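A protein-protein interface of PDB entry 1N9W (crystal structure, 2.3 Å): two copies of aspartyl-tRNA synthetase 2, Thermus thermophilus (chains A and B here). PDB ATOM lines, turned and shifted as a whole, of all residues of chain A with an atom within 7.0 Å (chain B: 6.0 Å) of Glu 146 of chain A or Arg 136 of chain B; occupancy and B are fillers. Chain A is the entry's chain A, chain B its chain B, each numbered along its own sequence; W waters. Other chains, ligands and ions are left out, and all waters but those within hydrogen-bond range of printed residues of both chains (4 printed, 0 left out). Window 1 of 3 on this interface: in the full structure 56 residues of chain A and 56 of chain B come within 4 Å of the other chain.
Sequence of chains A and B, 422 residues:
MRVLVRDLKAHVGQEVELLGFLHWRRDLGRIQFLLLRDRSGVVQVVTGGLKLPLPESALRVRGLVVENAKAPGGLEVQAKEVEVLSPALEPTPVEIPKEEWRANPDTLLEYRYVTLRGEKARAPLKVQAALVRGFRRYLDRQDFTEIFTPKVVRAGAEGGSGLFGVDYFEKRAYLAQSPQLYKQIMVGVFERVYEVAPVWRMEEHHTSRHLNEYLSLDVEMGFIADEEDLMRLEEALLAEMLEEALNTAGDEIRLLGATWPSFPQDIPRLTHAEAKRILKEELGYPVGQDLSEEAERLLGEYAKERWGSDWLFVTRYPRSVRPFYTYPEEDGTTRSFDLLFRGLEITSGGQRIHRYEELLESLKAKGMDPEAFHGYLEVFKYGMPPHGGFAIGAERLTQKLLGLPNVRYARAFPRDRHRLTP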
ATOM      1  N   VAL A 132      -7.557  12.508 -29.877  1.00  0.00           N
ATOM      2  CA  VAL A 132      -8.652  13.466 -30.044  1.00  0.00           C
ATOM      3  C   VAL A 132      -9.169  13.958 -28.687  1.00  0.00           C
ATOM      4  O   VAL A 132      -9.499  15.139 -28.541  1.00  0.00           O
ATOM      5  CB  VAL A 132      -9.809  12.845 -30.881  1.00  0.00           C
ATOM      6  CG1 VAL A 132     -10.857  13.900 -31.217  1.00  0.00           C
ATOM      7  CG2 VAL A 132      -9.236  12.249 -32.152  1.00  0.00           C
ATOM      8  N   ARG A 133      -9.226  13.072 -27.691  1.00  0.00           N
ATOM      9  CA  ARG A 133      -9.684  13.495 -26.364  1.00  0.00           C
ATOM     10  C   ARG A 133      -8.706  14.554 -25.823  1.00  0.00           C
ATOM     11  O   ARG A 133      -9.120  15.559 -25.242  1.00  0.00           O
ATOM     12  CB  ARG A 133      -9.748  12.303 -25.395  1.00  0.00           C
ATOM     13  CG  ARG A 133     -10.271  12.669 -23.997  1.00  0.00           C
ATOM     14  CD  ARG A 133     -10.104  11.502 -23.038  1.00  0.00           C
ATOM     15  NE  ARG A 133     -10.754  10.319 -23.561  1.00  0.00           N
ATOM     16  CZ  ARG A 133     -10.149   9.156 -23.771  1.00  0.00           C
ATOM     17  NH1 ARG A 133      -8.860   9.010 -23.496  1.00  0.00           N
ATOM     18  NH2 ARG A 133     -10.838   8.137 -24.277  1.00  0.00           N
ATOM     19  N   ARG A 136      -9.341  17.961 -27.723  1.00  0.00           N
ATOM     20  CA  ARG A 136     -10.461  18.739 -27.236  1.00  0.00           C
ATOM     21  C   ARG A 136     -10.219  19.274 -25.821  1.00  0.00           C
ATOM     22  O   ARG A 136     -10.559  20.421 -25.517  1.00  0.00           O
ATOM     23  CB  ARG A 136     -11.757  17.924 -27.255  1.00  0.00           C
ATOM     24  CG  ARG A 136     -12.226  17.491 -28.638  1.00  0.00           C
ATOM     25  CD  ARG A 136     -13.707  17.121 -28.598  1.00  0.00           C
ATOM     26  NE  ARG A 136     -14.135  16.398 -29.800  1.00  0.00           N
ATOM     27  CZ  ARG A 136     -14.090  15.078 -29.937  1.00  0.00           C
ATOM     28  NH1 ARG A 136     -13.639  14.318 -28.939  1.00  0.00           N
ATOM     29  NH2 ARG A 136     -14.488  14.524 -31.074  1.00  0.00           N
ATOM     30  N   ASP A 140     -10.343  23.102 -24.969  1.00  0.00           N
ATOM     31  CA  ASP A 140     -11.470  23.488 -24.103  1.00  0.00           C
ATOM     32  C   ASP A 140     -10.934  24.273 -22.904  1.00  0.00           C
ATOM     33  O   ASP A 140     -11.535  25.258 -22.474  1.00  0.00           O
ATOM     34  CB  ASP A 140     -12.235  22.250 -23.598  1.00  0.00           C
ATOM     35  CG  ASP A 140     -13.301  21.779 -24.562  1.00  0.00           C
ATOM     36  OD1 ASP A 140     -13.637  22.537 -25.496  1.00  0.00           O
ATOM     37  OD2 ASP A 140     -13.813  20.643 -24.371  1.00  0.00           O
ATOM     38  N   PHE A 144     -11.753  27.372 -25.809  1.00  0.00           N
ATOM     39  CA  PHE A 144     -12.177  27.216 -27.191  1.00  0.00           C
ATOM     40  C   PHE A 144     -13.580  26.611 -27.167  1.00  0.00           C
ATOM     41  O   PHE A 144     -13.914  25.851 -26.259  1.00  0.00           O
ATOM     42  CB  PHE A 144     -11.235  26.275 -27.952  1.00  0.00           C
ATOM     43  CG  PHE A 144     -10.002  26.942 -28.500  1.00  0.00           C
ATOM     44  CD1 PHE A 144      -9.017  27.451 -27.649  1.00  0.00           C
ATOM     45  CD2 PHE A 144      -9.810  27.029 -29.883  1.00  0.00           C
ATOM     46  CE1 PHE A 144      -7.859  28.032 -28.176  1.00  0.00           C
ATOM     47  CE2 PHE A 144      -8.663  27.607 -30.415  1.00  0.00           C
ATOM     48  CZ  PHE A 144      -7.676  28.112 -29.568  1.00  0.00           C
ATOM     49  N   THR A 145     -14.401  26.953 -28.151  1.00  0.00           N
ATOM     50  CA  THR A 145     -15.741  26.395 -28.225  1.00  0.00           C
ATOM     51  C   THR A 145     -15.731  25.418 -29.395  1.00  0.00           C
ATOM     52  O   THR A 145     -15.344  25.786 -30.503  1.00  0.00           O
ATOM     53  CB  THR A 145     -16.782  27.499 -28.504  1.00  0.00           C
ATOM     54  OG1 THR A 145     -16.680  28.512 -27.491  1.00  0.00           O
ATOM     55  CG2 THR A 145     -18.193  26.926 -28.514  1.00  0.00           C
ATOM     56  N   GLU A 146     -16.112  24.167 -29.162  1.00  0.00           N
ATOM     57  CA  GLU A 146     -16.156  23.202 -30.262  1.00  0.00           C
ATOM     58  C   GLU A 146     -17.384  23.570 -31.104  1.00  0.00           C
ATOM     59  O   GLU A 146     -18.433  23.893 -30.549  1.00  0.00           O
ATOM     60  CB  GLU A 146     -16.312  21.775 -29.736  1.00  0.00           C
ATOM     61  CG  GLU A 146     -16.635  20.745 -30.817  1.00  0.00           C
ATOM     62  CD  GLU A 146     -16.647  19.312 -30.285  1.00  0.00           C
ATOM     63  OE1 GLU A 146     -17.031  19.120 -29.108  1.00  0.00           O
ATOM     64  OE2 GLU A 146     -16.279  18.385 -31.046  1.00  0.00           O
ATOM     65  N   ILE A 147     -17.249  23.531 -32.427  1.00  0.00           N
ATOM     66  CA  ILE A 147     -18.353  23.874 -33.321  1.00  0.00           C
ATOM     67  C   ILE A 147     -18.665  22.744 -34.297  1.00  0.00           C
ATOM     68  O   ILE A 147     -17.870  21.812 -34.470  1.00  0.00           O
ATOM     69  CB  ILE A 147     -18.041  25.127 -34.155  1.00  0.00           C
ATOM     70  CG1 ILE A 147     -16.729  24.918 -34.926  1.00  0.00           C
ATOM     71  CG2 ILE A 147     -17.978  26.348 -33.257  1.00  0.00           C
ATOM     72  CD1 ILE A 147     -16.440  25.992 -35.971  1.00  0.00           C
ATOM     73  N   PHE A 148     -19.832  22.826 -34.926  1.00  0.00           N
ATOM     74  CA  PHE A 148     -20.223  21.815 -35.901  1.00  0.00           C
ATOM     75  C   PHE A 148     -20.763  22.519 -37.126  1.00  0.00           C
ATOM     76  O   PHE A 148     -21.859  23.079 -37.107  1.00  0.00           O
ATOM     77  CB  PHE A 148     -21.269  20.879 -35.289  1.00  0.00           C
ATOM     78  CG  PHE A 148     -20.870  20.335 -33.948  1.00  0.00           C
ATOM     79  CD1 PHE A 148     -21.076  21.088 -32.796  1.00  0.00           C
ATOM     80  CD2 PHE A 148     -20.233  19.101 -33.838  1.00  0.00           C
ATOM     81  CE1 PHE A 148     -20.659  20.617 -31.556  1.00  0.00           C
ATOM     82  CE2 PHE A 148     -19.813  18.621 -32.593  1.00  0.00           C
ATOM     83  CZ  PHE A 148     -20.023  19.377 -31.456  1.00  0.00           C
ATOM     84  N   PHE A 190     -17.171  33.255 -31.422  1.00  0.00           N
ATOM     85  CA  PHE A 190     -16.595  32.687 -30.199  1.00  0.00           C
ATOM     86  C   PHE A 190     -15.114  32.967 -29.946  1.00  0.00           C
ATOM     87  O   PHE A 190     -14.557  32.515 -28.941  1.00  0.00           O
ATOM     88  CB  PHE A 190     -16.828  31.166 -30.189  1.00  0.00           C
ATOM     89  CG  PHE A 190     -18.266  30.759 -29.987  1.00  0.00           C
ATOM     90  CD1 PHE A 190     -18.895  29.893 -30.879  1.00  0.00           C
ATOM     91  CD2 PHE A 190     -18.989  31.241 -28.896  1.00  0.00           C
ATOM     92  CE1 PHE A 190     -20.214  29.481 -30.670  1.00  0.00           C
ATOM     93  CE2 PHE A 190     -20.311  30.839 -28.676  1.00  0.00           C
ATOM     94  CZ  PHE A 190     -20.933  29.971 -29.571  1.00  0.00           C
ATOM     95  N   ARG A 192     -12.332  31.759 -30.444  1.00  0.00           N
ATOM     96  CA  ARG A 192     -11.448  30.606 -30.592  1.00  0.00           C
ATOM     97  C   ARG A 192     -12.346  29.390 -30.704  1.00  0.00           C
ATOM     98  O   ARG A 192     -13.202  29.149 -29.842  1.00  0.00           O
ATOM     99  CB  ARG A 192     -10.477  30.474 -29.391  1.00  0.00           C
ATOM    100  CG  ARG A 192     -10.862  31.257 -28.143  1.00  0.00           C
ATOM    101  CD  ARG A 192      -9.761  31.161 -27.078  1.00  0.00           C
ATOM    102  NE  ARG A 192      -8.571  31.932 -27.447  1.00  0.00           N
ATOM    103  CZ  ARG A 192      -7.412  31.888 -26.793  1.00  0.00           C
ATOM    104  NH1 ARG A 192      -7.262  31.109 -25.725  1.00  0.00           N
ATOM    105  NH2 ARG A 192      -6.398  32.628 -27.204  1.00  0.00           N
ATOM    106  N   VAL A 193     -12.179  28.649 -31.793  1.00  0.00           N
ATOM    107  CA  VAL A 193     -13.003  27.474 -32.039  1.00  0.00           C
ATOM    108  C   VAL A 193     -12.244  26.341 -32.704  1.00  0.00           C
ATOM    109  O   VAL A 193     -11.186  26.550 -33.301  1.00  0.00           O
ATOM    110  CB  VAL A 193     -14.178  27.796 -33.001  1.00  0.00           C
ATOM    111  CG1 VAL A 193     -14.991  28.976 -32.465  1.00  0.00           C
ATOM    112  CG2 VAL A 193     -13.652  28.062 -34.414  1.00  0.00           C
ATOM    113  N   TYR A 194     -12.799  25.140 -32.589  1.00  0.00           N
ATOM    114  CA  TYR A 194     -12.208  23.980 -33.228  1.00  0.00           C
ATOM    115  C   TYR A 194     -13.316  23.025 -33.673  1.00  0.00           C
ATOM    116  O   TYR A 194     -14.468  23.118 -33.229  1.00  0.00           O
ATOM    117  CB  TYR A 194     -11.229  23.252 -32.293  1.00  0.00           C
ATOM    118  CG  TYR A 194     -11.873  22.615 -31.088  1.00  0.00           C
ATOM    119  CD1 TYR A 194     -11.944  23.288 -29.867  1.00  0.00           C
ATOM    120  CD2 TYR A 194     -12.427  21.344 -31.169  1.00  0.00           C
ATOM    121  CE1 TYR A 194     -12.557  22.698 -28.753  1.00  0.00           C
ATOM    122  CE2 TYR A 194     -13.038  20.750 -30.073  1.00  0.00           C
ATOM    123  CZ  TYR A 194     -13.102  21.425 -28.871  1.00  0.00           C
ATOM    124  OH  TYR A 194     -13.709  20.818 -27.794  1.00  0.00           O
ATOM    125  N   GLU A 195     -12.959  22.123 -34.579  1.00  0.00           N
ATOM    126  CA  GLU A 195     -13.893  21.134 -35.087  1.00  0.00           C
ATOM    127  C   GLU A 195     -13.166  19.836 -35.392  1.00  0.00           C
ATOM    128  O   GLU A 195     -12.007  19.844 -35.812  1.00  0.00           O
ATOM    129  CB  GLU A 195     -14.580  21.634 -36.367  1.00  0.00           C
ATOM    130  CG  GLU A 195     -15.606  20.652 -36.928  1.00  0.00           C
ATOM    131  CD  GLU A 195     -16.513  21.272 -37.987  1.00  0.00           C
ATOM    132  OE1 GLU A 195     -17.575  20.690 -38.291  1.00  0.00           O
ATOM    133  OE2 GLU A 195     -16.159  22.344 -38.512  1.00  0.00           O
ATOM    134  N   VAL A 196     -13.852  18.719 -35.169  1.00  0.00           N
ATOM    135  CA  VAL A 196     -13.310  17.386 -35.446  1.00  0.00           C
ATOM    136  C   VAL A 196     -14.273  16.763 -36.448  1.00  0.00           C
ATOM    137  O   VAL A 196     -15.406  16.442 -36.096  1.00  0.00           O
ATOM    138  CB  VAL A 196     -13.307  16.481 -34.189  1.00  0.00           C
ATOM    139  CG1 VAL A 196     -12.720  15.112 -34.544  1.00  0.00           C
ATOM    140  CG2 VAL A 196     -12.531  17.129 -33.073  1.00  0.00           C
ATOM    141  N   LEU B 125     -25.472  27.537 -29.109  1.00  0.00           N
ATOM    142  CA  LEU B 125     -24.360  26.756 -29.639  1.00  0.00           C
ATOM    143  C   LEU B 125     -23.328  26.481 -28.538  1.00  0.00           C
ATOM    144  O   LEU B 125     -22.696  25.422 -28.513  1.00  0.00           O
ATOM    145  CB  LEU B 125     -23.704  27.497 -30.823  1.00  0.00           C
ATOM    146  CG  LEU B 125     -24.581  27.768 -32.058  1.00  0.00           C
ATOM    147  CD1 LEU B 125     -23.785  28.501 -33.134  1.00  0.00           C
ATOM    148  CD2 LEU B 125     -25.103  26.443 -32.614  1.00  0.00           C
ATOM    149  N   ALA B 129     -22.254  22.764 -27.150  1.00  0.00           N
ATOM    150  CA  ALA B 129     -20.887  22.297 -27.034  1.00  0.00           C
ATOM    151  C   ALA B 129     -20.698  21.708 -25.650  1.00  0.00           C
ATOM    152  O   ALA B 129     -19.979  20.721 -25.471  1.00  0.00           O
ATOM    153  CB  ALA B 129     -19.897  23.439 -27.266  1.00  0.00           C
ATOM    154  N   LEU B 131     -23.130  20.305 -23.747  1.00  0.00           N
ATOM    155  CA  LEU B 131     -23.856  19.017 -23.719  1.00  0.00           C
ATOM    156  C   LEU B 131     -23.054  17.884 -24.363  1.00  0.00           C
ATOM    157  O   LEU B 131     -23.021  16.765 -23.852  1.00  0.00           O
ATOM    158  CB  LEU B 131     -25.196  19.144 -24.451  1.00  0.00           C
ATOM    159  CG  LEU B 131     -26.224  20.112 -23.849  1.00  0.00           C
ATOM    160  CD1 LEU B 131     -27.315  20.390 -24.861  1.00  0.00           C
ATOM    161  CD2 LEU B 131     -26.801  19.530 -22.559  1.00  0.00           C
ATOM    162  N   VAL B 132     -22.420  18.172 -25.492  1.00  0.00           N
ATOM    163  CA  VAL B 132     -21.635  17.160 -26.185  1.00  0.00           C
ATOM    164  C   VAL B 132     -20.392  16.783 -25.372  1.00  0.00           C
ATOM    165  O   VAL B 132     -19.978  15.615 -25.358  1.00  0.00           O
ATOM    166  CB  VAL B 132     -21.236  17.670 -27.589  1.00  0.00           C
ATOM    167  CG1 VAL B 132     -20.303  16.686 -28.269  1.00  0.00           C
ATOM    168  CG2 VAL B 132     -22.491  17.876 -28.430  1.00  0.00           C
ATOM    169  N   ARG B 133     -19.796  17.763 -24.693  1.00  0.00           N
ATOM    170  CA  ARG B 133     -18.618  17.502 -23.871  1.00  0.00           C
ATOM    171  C   ARG B 133     -19.028  16.532 -22.752  1.00  0.00           C
ATOM    172  O   ARG B 133     -18.312  15.571 -22.455  1.00  0.00           O
ATOM    173  CB  ARG B 133     -18.077  18.815 -23.269  1.00  0.00           C
ATOM    174  CG  ARG B 133     -16.815  18.676 -22.399  1.00  0.00           C
ATOM    175  CD  ARG B 133     -16.496  20.010 -21.701  1.00  0.00           C
ATOM    176  NE  ARG B 133     -16.372  21.077 -22.685  1.00  0.00           N
ATOM    177  CZ  ARG B 133     -16.935  22.276 -22.589  1.00  0.00           C
ATOM    178  NH1 ARG B 133     -17.674  22.595 -21.533  1.00  0.00           N
ATOM    179  NH2 ARG B 133     -16.785  23.150 -23.578  1.00  0.00           N
ATOM    180  N   GLY B 134     -20.194  16.783 -22.155  1.00  0.00           N
ATOM    181  CA  GLY B 134     -20.695  15.920 -21.093  1.00  0.00           C
ATOM    182  C   GLY B 134     -20.963  14.529 -21.622  1.00  0.00           C
ATOM    183  O   GLY B 134     -20.723  13.527 -20.947  1.00  0.00           O
ATOM    184  N   PHE B 135     -21.465  14.482 -22.850  1.00  0.00           N
ATOM    185  CA  PHE B 135     -21.784  13.236 -23.533  1.00  0.00           C
ATOM    186  C   PHE B 135     -20.546  12.349 -23.612  1.00  0.00           C
ATOM    187  O   PHE B 135     -20.569  11.197 -23.183  1.00  0.00           O
ATOM    188  CB  PHE B 135     -22.279  13.565 -24.939  1.00  0.00           C
ATOM    189  CG  PHE B 135     -22.609  12.369 -25.776  1.00  0.00           C
ATOM    190  CD1 PHE B 135     -23.811  11.686 -25.596  1.00  0.00           C
ATOM    191  CD2 PHE B 135     -21.725  11.930 -26.759  1.00  0.00           C
ATOM    192  CE1 PHE B 135     -24.128  10.590 -26.388  1.00  0.00           C
ATOM    193  CE2 PHE B 135     -22.031  10.833 -27.556  1.00  0.00           C
ATOM    194  CZ  PHE B 135     -23.235  10.157 -27.374  1.00  0.00           C
ATOM    195  N   ARG B 136     -19.461  12.901 -24.160  1.00  0.00           N
ATOM    196  CA  ARG B 136     -18.210  12.163 -24.311  1.00  0.00           C
ATOM    197  C   ARG B 136     -17.534  11.802 -22.980  1.00  0.00           C
ATOM    198  O   ARG B 136     -16.935  10.731 -22.858  1.00  0.00           O
ATOM    199  CB  ARG B 136     -17.222  12.957 -25.178  1.00  0.00           C
ATOM    200  CG  ARG B 136     -17.717  13.300 -26.581  1.00  0.00           C
ATOM    201  CD  ARG B 136     -16.531  13.435 -27.549  1.00  0.00           C
ATOM    202  NE  ARG B 136     -16.880  14.026 -28.847  1.00  0.00           N
ATOM    203  CZ  ARG B 136     -17.016  15.330 -29.068  1.00  0.00           C
ATOM    204  NH1 ARG B 136     -16.829  16.195 -28.077  1.00  0.00           N
ATOM    205  NH2 ARG B 136     -17.342  15.770 -30.283  1.00  0.00           N
ATOM    206  N   ARG B 137     -17.623  12.693 -21.996  1.00  0.00           N
ATOM    207  CA  ARG B 137     -17.012  12.453 -20.694  1.00  0.00           C
ATOM    208  C   ARG B 137     -17.676  11.262 -20.008  1.00  0.00           C
ATOM    209  O   ARG B 137     -16.998  10.313 -19.620  1.00  0.00           O
ATOM    210  CB  ARG B 137     -17.141  13.691 -19.792  1.00  0.00           C
ATOM    211  CG  ARG B 137     -16.170  13.715 -18.603  1.00  0.00           C
ATOM    212  CD  ARG B 137     -16.603  14.656 -17.468  1.00  0.00           C
ATOM    213  NE  ARG B 137     -16.628  16.085 -17.799  1.00  0.00           N
ATOM    214  CZ  ARG B 137     -15.573  16.808 -18.180  1.00  0.00           C
ATOM    215  NH1 ARG B 137     -14.382  16.241 -18.295  1.00  0.00           N
ATOM    216  NH2 ARG B 137     -15.702  18.108 -18.417  1.00  0.00           N
ATOM    217  N   TYR B 138     -18.997  11.308 -19.864  1.00  0.00           N
ATOM    218  CA  TYR B 138     -19.705  10.218 -19.202  1.00  0.00           C
ATOM    219  C   TYR B 138     -19.384   8.874 -19.838  1.00  0.00           C
ATOM    220  O   TYR B 138     -19.045   7.926 -19.142  1.00  0.00           O
ATOM    221  CB  TYR B 138     -21.225  10.432 -19.235  1.00  0.00           C
ATOM    222  CG  TYR B 138     -21.977   9.255 -18.645  1.00  0.00           C
ATOM    223  CD1 TYR B 138     -22.043   9.060 -17.261  1.00  0.00           C
ATOM    224  CD2 TYR B 138     -22.531   8.276 -19.475  1.00  0.00           C
ATOM    225  CE1 TYR B 138     -22.628   7.910 -16.721  1.00  0.00           C
ATOM    226  CE2 TYR B 138     -23.115   7.125 -18.948  1.00  0.00           C
ATOM    227  CZ  TYR B 138     -23.158   6.952 -17.568  1.00  0.00           C
ATOM    228  OH  TYR B 138     -23.704   5.809 -17.042  1.00  0.00           O
ATOM    229  N   LEU B 139     -19.486   8.798 -21.160  1.00  0.00           N
ATOM    230  CA  LEU B 139     -19.207   7.549 -21.857  1.00  0.00           C
ATOM    231  C   LEU B 139     -17.733   7.133 -21.757  1.00  0.00           C
ATOM    232  O   LEU B 139     -17.437   5.947 -21.581  1.00  0.00           O
ATOM    233  CB  LEU B 139     -19.655   7.651 -23.321  1.00  0.00           C
ATOM    234  CG  LEU B 139     -21.182   7.817 -23.508  1.00  0.00           C
ATOM    235  CD1 LEU B 139     -21.495   8.189 -24.954  1.00  0.00           C
ATOM    236  CD2 LEU B 139     -21.915   6.517 -23.104  1.00  0.00           C
ATOM    237  N   ASP B 140     -16.806   8.087 -21.869  1.00  0.00           N
ATOM    238  CA  ASP B 140     -15.376   7.760 -21.745  1.00  0.00           C
ATOM    239  C   ASP B 140     -15.107   7.138 -20.370  1.00  0.00           C
ATOM    240  O   ASP B 140     -14.334   6.194 -20.259  1.00  0.00           O
ATOM    241  CB  ASP B 140     -14.484   9.011 -21.888  1.00  0.00           C
ATOM    242  CG  ASP B 140     -14.290   9.457 -23.340  1.00  0.00           C
ATOM    243  OD1 ASP B 140     -14.551   8.655 -24.272  1.00  0.00           O
ATOM    244  OD2 ASP B 140     -13.853  10.618 -23.542  1.00  0.00           O
ATOM    245  N   ARG B 141     -15.731   7.683 -19.326  1.00  0.00           N
ATOM    246  CA  ARG B 141     -15.537   7.154 -17.982  1.00  0.00           C
ATOM    247  C   ARG B 141     -16.115   5.740 -17.819  1.00  0.00           C
ATOM    248  O   ARG B 141     -15.726   5.018 -16.900  1.00  0.00           O
ATOM    249  CB  ARG B 141     -16.140   8.097 -16.941  1.00  0.00           C
ATOM    250  CG  ARG B 141     -15.811   7.731 -15.497  1.00  0.00           C
ATOM    251  CD  ARG B 141     -15.990   8.933 -14.585  1.00  0.00           C
ATOM    252  NE  ARG B 141     -17.274   9.566 -14.851  1.00  0.00           N
ATOM    253  CZ  ARG B 141     -17.442  10.857 -15.123  1.00  0.00           C
ATOM    254  NH1 ARG B 141     -16.404  11.685 -15.161  1.00  0.00           N
ATOM    255  NH2 ARG B 141     -18.659  11.315 -15.379  1.00  0.00           N
ATOM    256  N   GLU B 146     -14.534   6.375 -28.585  1.00  0.00           N
ATOM    257  CA  GLU B 146     -15.062   7.223 -29.654  1.00  0.00           C
ATOM    258  C   GLU B 146     -14.573   6.686 -30.991  1.00  0.00           C
ATOM    259  O   GLU B 146     -13.395   6.355 -31.144  1.00  0.00           O
ATOM    260  CB  GLU B 146     -14.602   8.678 -29.478  1.00  0.00           C
ATOM    261  CG  GLU B 146     -14.964   9.610 -30.642  1.00  0.00           C
ATOM    262  CD  GLU B 146     -14.898  11.090 -30.275  1.00  0.00           C
ATOM    263  OE1 GLU B 146     -14.000  11.481 -29.498  1.00  0.00           O
ATOM    264  OE2 GLU B 146     -15.741  11.867 -30.781  1.00  0.00           O
ATOM    265  N   TYR B 194     -19.211   5.103 -29.332  1.00  0.00           N
ATOM    266  CA  TYR B 194     -20.136   6.188 -29.582  1.00  0.00           C
ATOM    267  C   TYR B 194     -19.565   7.061 -30.672  1.00  0.00           C
ATOM    268  O   TYR B 194     -18.379   6.979 -31.001  1.00  0.00           O
ATOM    269  CB  TYR B 194     -20.368   7.032 -28.326  1.00  0.00           C
ATOM    270  CG  TYR B 194     -19.161   7.820 -27.874  1.00  0.00           C
ATOM    271  CD1 TYR B 194     -18.258   7.289 -26.958  1.00  0.00           C
ATOM    272  CD2 TYR B 194     -18.939   9.116 -28.349  1.00  0.00           C
ATOM    273  CE1 TYR B 194     -17.164   8.031 -26.518  1.00  0.00           C
ATOM    274  CE2 TYR B 194     -17.852   9.865 -27.917  1.00  0.00           C
ATOM    275  CZ  TYR B 194     -16.969   9.316 -26.996  1.00  0.00           C
ATOM    276  OH  TYR B 194     -15.910  10.060 -26.531  1.00  0.00           O
ATOM    277  N   VAL B 196     -20.091  11.131 -32.674  1.00  0.00           N
ATOM    278  CA  VAL B 196     -20.695  12.444 -32.788  1.00  0.00           C
ATOM    279  C   VAL B 196     -20.479  12.879 -34.218  1.00  0.00           C
ATOM    280  O   VAL B 196     -19.371  13.257 -34.592  1.00  0.00           O
ATOM    281  CB  VAL B 196     -19.989  13.449 -31.870  1.00  0.00           C
ATOM    282  CG1 VAL B 196     -20.557  14.838 -32.082  1.00  0.00           C
ATOM    283  CG2 VAL B 196     -20.124  13.005 -30.426  1.00  0.00           C
ATOM    284  N   LEU B 237     -26.490   9.257 -18.738  1.00  0.00           N
ATOM    285  CA  LEU B 237     -25.798  10.039 -19.753  1.00  0.00           C
ATOM    286  C   LEU B 237     -26.371  11.457 -19.792  1.00  0.00           C
ATOM    287  O   LEU B 237     -25.630  12.436 -19.725  1.00  0.00           O
ATOM    288  CB  LEU B 237     -25.961   9.379 -21.127  1.00  0.00           C
ATOM    289  CG  LEU B 237     -25.451  10.119 -22.372  1.00  0.00           C
ATOM    290  CD1 LEU B 237     -23.940  10.247 -22.316  1.00  0.00           C
ATOM    291  CD2 LEU B 237     -25.880   9.354 -23.624  1.00  0.00           C
HETATM  292  O   HOH W   1     -16.071  22.889 -26.467  1.00  0.00           O
HETATM  293  O   HOH W   2     -16.548  14.987 -33.102  1.00  0.00           O
HETATM  294  O   HOH W   3     -12.996   7.991 -26.525  1.00  0.00           O
HETATM  295  O   HOH W   4     -17.324  20.231 -26.814  1.00  0.00           O
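Of the 17 printed residues of chain B, 7 touch a printed residue of chain A.
Hydrophobic or aromatic side chains of chain B within 4 Å of the printed part of chain A: Leu 125, Ala 129 and Val 196.
Along chain B the printed residues that touch a printed residue of chain A span positions 125 to 196.
Among the printed residues, 8 pairs touch across the chains.
Among the printed residues, Asp or Glu carboxylates within 4 Å of a Lys or Arg side-chain nitrogen of the other chain: Arg 133 of chain A with Asp 140 of chain B (3.1 Å), Arg 136 of chain A with Glu 146 of chain B (2.9 Å), Asp 140 of chain A with Arg 133 of chain B (3.1 Å) and Glu 146 of chain A with Arg 136 of chain B (2.9 Å).
Water W3 lies within hydrogen-bond range of the side-chain carboxylate of Asp 140 of chain B, the backbone NH of Glu 146 of chain B and the guanidinium group of Arg 133 of chain A.
Water W2 lies within hydrogen-bond range of the guanidinium group (NH2) of Arg 136 of chain A (2.9 Å) and the guanidinium group (NH2) of Arg 136 of chain B (3.0 Å).
OD1 of Asp 140 of chain B sits at hydrogen-bond distance from OH of Tyr 194 of chain B (3.0 Å).
OD1 of Asp 140 of chain A lies within hydrogen-bond range of OH of Tyr 194 of chain A, at 2.9 Å.
OE2 of Glu 146 of chain A is in salt-bridge range of NE of Arg 136 of chain A, at 3.2 Å.
The guanidinium group of Arg 136 of chain B is in salt-bridge range of the side-chain carboxylate of Glu 146 of chain B, at 3.1 Å.
Glu 146 of chain A touches Ala 129 of chain B.
Phe 148 of chain A touches Val 196 of chain B.
CZ of Phe 190 of chain A touches CB of Leu 125 of chain B (3.9 Å).
Of chain B, only Ala 129 and Arg 136 come within 4 Å of Glu 146 of chain A.
Of chain A, only Arg 136 (3.1 Å) and Glu 146 (2.9 Å) come within 4 Å of Arg 136 of chain B.
Printed residues of chain B within 4 Å of Phe 148 of chain A: Val 196 (3.9 Å).
Of the printed residues of chain B, Arg 136 of chain A touches Arg 136 and Glu 146.
Printed residues of chain A within 4 Å of Leu 125 of chain B: Phe 190.
Leu 131 of chain B touches none of the printed residues of chain A.
Arg 137 of chain B touches none of the printed residues of chain A.
The nearest residue of chain B that does not touch Glu 146 of chain A is Val 132 of chain B (4.2 Å).
Arg 133 of chain A touches Asp 140 of chain B, and with the chains exchanged Asp 140 of chain A touches Arg 133 of chain B.
Arg 136 of chain B touches its own counterpart, Arg 136 of chain A.
Arg 136 of chain A touches Glu 146 of chain B, and with the chains exchanged Glu 146 of chain A touches Arg 136 of chain B.
OD2 of Asp 140 of chain B lies within salt-bridge range of NE of Arg 133 of chain A, 3.1 Å away.
NH1 of Arg 136 of chain A lies within salt-bridge range of OE1 of Glu 146 of chain B, 2.9 Å away.
NH2 of Arg 136 of chain B is in salt-bridge range of OE2 of Glu 146 of chain A.
The side-chain carboxylate of Asp 140 of chain A lies within salt-bridge range of the guanidinium group of Arg 133 of chain B (3.1 Å).
The guanidinium group (NH1) of Arg 136 of chain B sits close to the guanidinium group (NE) of Arg 136 of chain A (3.2 Å).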
